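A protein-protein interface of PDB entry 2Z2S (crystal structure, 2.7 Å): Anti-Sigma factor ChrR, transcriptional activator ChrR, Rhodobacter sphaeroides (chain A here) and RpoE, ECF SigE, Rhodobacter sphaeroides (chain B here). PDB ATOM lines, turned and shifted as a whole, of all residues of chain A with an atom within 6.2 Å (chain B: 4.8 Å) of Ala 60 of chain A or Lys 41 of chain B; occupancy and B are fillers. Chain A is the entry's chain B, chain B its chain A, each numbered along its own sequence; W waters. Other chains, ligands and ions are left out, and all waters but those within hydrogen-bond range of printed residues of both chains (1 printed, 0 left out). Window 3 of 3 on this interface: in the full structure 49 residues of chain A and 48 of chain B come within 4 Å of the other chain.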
ATOM      1  N   PRO A  58     -23.967 -18.718  -8.469  1.00  0.00           N
ATOM      2  CA  PRO A  58     -24.030 -17.483  -9.244  1.00  0.00           C
ATOM      3  C   PRO A  58     -22.769 -17.218 -10.055  1.00  0.00           C
ATOM      4  O   PRO A  58     -21.707 -17.737  -9.753  1.00  0.00           O
ATOM      5  CB  PRO A  58     -24.304 -16.426  -8.176  1.00  0.00           C
ATOM      6  CG  PRO A  58     -23.631 -17.000  -6.990  1.00  0.00           C
ATOM      7  CD  PRO A  58     -24.056 -18.430  -7.031  1.00  0.00           C
ATOM      8  N   VAL A  59     -22.916 -16.419 -11.102  1.00  0.00           N
ATOM      9  CA  VAL A  59     -21.820 -16.060 -11.984  1.00  0.00           C
ATOM     10  C   VAL A  59     -21.897 -14.539 -12.114  1.00  0.00           C
ATOM     11  O   VAL A  59     -22.876 -13.994 -12.623  1.00  0.00           O
ATOM     12  CB  VAL A  59     -21.983 -16.758 -13.360  1.00  0.00           C
ATOM     13  CG1 VAL A  59     -21.034 -16.151 -14.385  1.00  0.00           C
ATOM     14  CG2 VAL A  59     -21.719 -18.270 -13.200  1.00  0.00           C
ATOM     15  N   ALA A  60     -20.864 -13.859 -11.639  1.00  0.00           N
ATOM     16  CA  ALA A  60     -20.860 -12.417 -11.652  1.00  0.00           C
ATOM     17  C   ALA A  60     -21.041 -11.828 -13.038  1.00  0.00           C
ATOM     18  O   ALA A  60     -20.611 -12.421 -14.034  1.00  0.00           O
ATOM     19  CB  ALA A  60     -19.585 -11.924 -11.046  1.00  0.00           C
ATOM     20  N   LEU A  61     -21.706 -10.677 -13.107  1.00  0.00           N
ATOM     21  CA  LEU A  61     -21.891  -9.992 -14.380  1.00  0.00           C
ATOM     22  C   LEU A  61     -20.777  -8.970 -14.458  1.00  0.00           C
ATOM     23  O   LEU A  61     -20.185  -8.618 -13.443  1.00  0.00           O
ATOM     24  CB  LEU A  61     -23.236  -9.267 -14.460  1.00  0.00           C
ATOM     25  CG  LEU A  61     -24.456 -10.106 -14.823  1.00  0.00           C
ATOM     26  CD1 LEU A  61     -24.947 -10.869 -13.589  1.00  0.00           C
ATOM     27  CD2 LEU A  61     -25.541  -9.199 -15.348  1.00  0.00           C
ATOM     28  N   SER A  62     -20.474  -8.493 -15.656  1.00  0.00           N
ATOM     29  CA  SER A  62     -19.419  -7.511 -15.778  1.00  0.00           C
ATOM     30  C   SER A  62     -19.839  -6.323 -14.920  1.00  0.00           C
ATOM     31  O   SER A  62     -21.036  -6.048 -14.777  1.00  0.00           O
ATOM     32  CB  SER A  62     -19.254  -7.097 -17.246  1.00  0.00           C
ATOM     33  OG  SER A  62     -20.375  -6.366 -17.725  1.00  0.00           O
ATOM     34  N   ALA B  37     -29.802 -11.730 -10.890  1.00  0.00           N
ATOM     35  CA  ALA B  37     -29.106 -11.603 -12.175  1.00  0.00           C
ATOM     36  C   ALA B  37     -27.974 -12.607 -12.353  1.00  0.00           C
ATOM     37  O   ALA B  37     -27.915 -13.308 -13.364  1.00  0.00           O
ATOM     38  CB  ALA B  37     -28.556 -10.162 -12.374  1.00  0.00           C
ATOM     39  N   PRO B  38     -27.056 -12.687 -11.378  1.00  0.00           N
ATOM     40  CA  PRO B  38     -25.935 -13.622 -11.478  1.00  0.00           C
ATOM     41  C   PRO B  38     -26.398 -15.069 -11.524  1.00  0.00           C
ATOM     42  O   PRO B  38     -25.747 -15.918 -12.114  1.00  0.00           O
ATOM     43  CB  PRO B  38     -25.117 -13.317 -10.225  1.00  0.00           C
ATOM     44  CG  PRO B  38     -25.454 -11.907  -9.943  1.00  0.00           C
ATOM     45  CD  PRO B  38     -26.935 -11.877 -10.161  1.00  0.00           C
ATOM     46  N   LYS B  39     -27.527 -15.350 -10.893  1.00  0.00           N
ATOM     47  CA  LYS B  39     -28.051 -16.702 -10.887  1.00  0.00           C
ATOM     48  C   LYS B  39     -28.673 -17.026 -12.236  1.00  0.00           C
ATOM     49  O   LYS B  39     -28.541 -18.141 -12.725  1.00  0.00           O
ATOM     50  CB  LYS B  39     -29.059 -16.864  -9.745  1.00  0.00           C
ATOM     51  CG  LYS B  39     -28.369 -17.072  -8.406  1.00  0.00           C
ATOM     52  CD  LYS B  39     -29.350 -17.113  -7.252  1.00  0.00           C
ATOM     53  CE  LYS B  39     -28.711 -17.759  -6.037  1.00  0.00           C
ATOM     54  NZ  LYS B  39     -28.231 -19.104  -6.415  1.00  0.00           N
ATOM     55  N   VAL B  40     -29.330 -16.043 -12.841  1.00  0.00           N
ATOM     56  CA  VAL B  40     -29.941 -16.221 -14.147  1.00  0.00           C
ATOM     57  C   VAL B  40     -28.859 -16.442 -15.177  1.00  0.00           C
ATOM     58  O   VAL B  40     -29.064 -17.132 -16.172  1.00  0.00           O
ATOM     59  CB  VAL B  40     -30.741 -15.002 -14.550  1.00  0.00           C
ATOM     60  CG1 VAL B  40     -31.037 -15.047 -16.036  1.00  0.00           C
ATOM     61  CG2 VAL B  40     -32.032 -14.990 -13.777  1.00  0.00           C
ATOM     62  N   LYS B  41     -27.700 -15.848 -14.932  1.00  0.00           N
ATOM     63  CA  LYS B  41     -26.581 -15.985 -15.847  1.00  0.00           C
ATOM     64  C   LYS B  41     -25.993 -17.376 -15.728  1.00  0.00           C
ATOM     65  O   LYS B  41     -25.886 -18.105 -16.715  1.00  0.00           O
ATOM     66  CB  LYS B  41     -25.507 -14.939 -15.534  1.00  0.00           C
ATOM     67  CG  LYS B  41     -24.260 -15.037 -16.396  1.00  0.00           C
ATOM     68  CD  LYS B  41     -23.298 -13.900 -16.104  1.00  0.00           C
ATOM     69  CE  LYS B  41     -21.996 -14.099 -16.839  1.00  0.00           C
ATOM     70  NZ  LYS B  41     -21.307 -12.799 -17.047  1.00  0.00           N
ATOM     71  N   GLY B  42     -25.618 -17.740 -14.509  1.00  0.00           N
ATOM     72  CA  GLY B  42     -25.034 -19.046 -14.292  1.00  0.00           C
ATOM     73  C   GLY B  42     -25.955 -20.130 -14.787  1.00  0.00           C
ATOM     74  O   GLY B  42     -25.520 -21.126 -15.356  1.00  0.00           O
ATOM     75  N   PHE B  43     -27.244 -19.935 -14.562  1.00  0.00           N
ATOM     76  CA  PHE B  43     -28.228 -20.905 -14.995  1.00  0.00           C
ATOM     77  C   PHE B  43     -28.185 -21.072 -16.511  1.00  0.00           C
ATOM     78  O   PHE B  43     -28.055 -22.187 -17.004  1.00  0.00           O
ATOM     79  CB  PHE B  43     -29.623 -20.456 -14.599  1.00  0.00           C
ATOM     80  CG  PHE B  43     -30.691 -21.432 -14.969  1.00  0.00           C
ATOM     81  CD1 PHE B  43     -30.895 -22.576 -14.209  1.00  0.00           C
ATOM     82  CD2 PHE B  43     -31.493 -21.212 -16.078  1.00  0.00           C
ATOM     83  CE1 PHE B  43     -31.878 -23.485 -14.536  1.00  0.00           C
ATOM     84  CE2 PHE B  43     -32.481 -22.121 -16.415  1.00  0.00           C
ATOM     85  CZ  PHE B  43     -32.673 -23.261 -15.635  1.00  0.00           C
ATOM     86  N   LEU B  44     -28.301 -19.965 -17.243  1.00  0.00           N
ATOM     87  CA  LEU B  44     -28.293 -20.008 -18.698  1.00  0.00           C
ATOM     88  C   LEU B  44     -27.026 -20.621 -19.274  1.00  0.00           C
ATOM     89  O   LEU B  44     -27.064 -21.210 -20.349  1.00  0.00           O
ATOM     90  CB  LEU B  44     -28.511 -18.611 -19.271  1.00  0.00           C
ATOM     91  CG  LEU B  44     -29.959 -18.166 -19.196  1.00  0.00           C
ATOM     92  CD1 LEU B  44     -30.133 -16.822 -19.843  1.00  0.00           C
ATOM     93  CD2 LEU B  44     -30.800 -19.183 -19.909  1.00  0.00           C
ATOM     94  N   MET B  45     -25.908 -20.474 -18.563  1.00  0.00           N
ATOM     95  CA  MET B  45     -24.643 -21.049 -18.998  1.00  0.00           C
ATOM     96  C   MET B  45     -24.659 -22.554 -18.782  1.00  0.00           C
ATOM     97  O   MET B  45     -24.178 -23.300 -19.628  1.00  0.00           O
ATOM     98  CB  MET B  45     -23.474 -20.421 -18.246  1.00  0.00           C
ATOM     99  CG  MET B  45     -23.081 -19.058 -18.799  1.00  0.00           C
ATOM    100  SD  MET B  45     -21.628 -18.189 -17.823  1.00  0.00           S
ATOM    101  CE  MET B  45     -20.513 -19.747 -17.507  1.00  0.00           C
ATOM    102  N   ALA B  51     -20.959 -17.125 -21.802  1.00  0.00           N
ATOM    103  CA  ALA B  51     -21.014 -16.050 -20.824  1.00  0.00           C
ATOM    104  C   ALA B  51     -21.657 -14.774 -21.375  1.00  0.00           C
ATOM    105  O   ALA B  51     -22.728 -14.362 -20.918  1.00  0.00           O
ATOM    106  CB  ALA B  51     -19.615 -15.751 -20.300  1.00  0.00           C
ATOM    107  N   ALA B  54     -25.154 -14.962 -22.054  1.00  0.00           N
ATOM    108  CA  ALA B  54     -25.901 -15.194 -20.821  1.00  0.00           C
ATOM    109  C   ALA B  54     -26.179 -13.854 -20.143  1.00  0.00           C
ATOM    110  O   ALA B  54     -27.330 -13.506 -19.860  1.00  0.00           O
ATOM    111  CB  ALA B  54     -25.108 -16.104 -19.890  1.00  0.00           C
ATOM    112  N   GLU B  55     -25.105 -13.113 -19.894  1.00  0.00           N
ATOM    113  CA  GLU B  55     -25.192 -11.808 -19.274  1.00  0.00           C
ATOM    114  C   GLU B  55     -26.166 -10.940 -20.060  1.00  0.00           C
ATOM    115  O   GLU B  55     -26.888 -10.132 -19.492  1.00  0.00           O
ATOM    116  CB  GLU B  55     -23.804 -11.176 -19.234  1.00  0.00           C
ATOM    117  CG  GLU B  55     -23.799  -9.717 -18.836  1.00  0.00           C
ATOM    118  CD  GLU B  55     -22.467  -9.273 -18.255  1.00  0.00           C
ATOM    119  OE1 GLU B  55     -22.247  -8.040 -18.134  1.00  0.00           O
ATOM    120  OE2 GLU B  55     -21.651 -10.165 -17.912  1.00  0.00           O
ATOM    121  N   ALA B  58     -29.538 -12.351 -19.013  1.00  0.00           N
ATOM    122  CA  ALA B  58     -29.753 -12.034 -17.615  1.00  0.00           C
ATOM    123  C   ALA B  58     -30.345 -10.619 -17.534  1.00  0.00           C
ATOM    124  O   ALA B  58     -31.488 -10.430 -17.100  1.00  0.00           O
ATOM    125  CB  ALA B  58     -28.438 -12.111 -16.876  1.00  0.00           C
HETATM  126  O   HOH W   1     -18.576 -10.166 -16.378  1.00  0.00           O
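Pro 58 of chain A touches Pro 38 of chain B (CA to O, 3.7 Å).
Val 59 of chain A touches Lys 41 of chain B.
Val 59 of chain A touches Gly 42 of chain B.
Ala 37 of chain B touches Leu 61 of chain A (C to CD1, 3.7 Å).
Leu 61 of chain A touches Pro 38 of chain B (CD1 to N, 3.6 Å).
Lys 41 of chain B touches Leu 61 of chain A.
OE2 of Glu 55 of chain B touches CA of Leu 61 of chain A (3.5 Å).
Water W1 lies within hydrogen-bond range of the backbone NH of Ser 62 of chain A (2.6 Å) and the side-chain carboxylate of Glu 55 of chain B (3.4 Å).
OE1 of Glu 55 of chain B sits at hydrogen-bond distance from OG of Ser 62 of chain A (2.5 Å).
The side-chain amino group (NZ) of Lys 41 of chain B sits at hydrogen-bond distance from the backbone carbonyl oxygen (O) of Ala 60 of chain A (3.1 Å).
The backbone NH of Val 59 of chain A lies within hydrogen-bond range of the backbone carbonyl oxygen of Pro 38 of chain B.
NZ of Lys 41 of chain B lies within salt-bridge range of OE2 of Glu 55 of chain B (2.8 Å).
Of the 5 printed residues of chain A, 5 touch a printed residue of chain B.
Hydrophobic or aromatic side chains of chain A within 4 Å of the printed part of chain B: Pro 58, Val 59 and Leu 61.
Among the printed residues, 10 pairs touch across the chains.
Ala 60 of chain A touches just one residue of chain B: Lys 41 (3.1 Å).
Lys 41 of chain B touches just these residues of chain A: Val 59, Ala 60 and Leu 61.
Printed residues of chain B within 4 Å of Pro 58 of chain A: Pro 38.
Printed residues of chain A within 4 Å of Pro 38 of chain B: Pro 58, Val 59 and Leu 61.
Printed residues of chain B within 4 Å of Ser 62 of chain A: Glu 55 (2.5 Å).
Printed residues of chain B within 4 Å of Leu 61 of chain A: Ala 37, Pro 38, Lys 41 and Glu 55.
The nearest residue of chain B that does not touch Ala 60 of chain A is Pro 38 of chain B (4.5 Å).
The nearest residue of chain A that does not touch Lys 41 of chain B is Ser 62 of chain A (4.6 Å).
The nearest printed residue of chain A that does not touch Ala 37 of chain B is Val 59 of chain A (5.1 Å).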
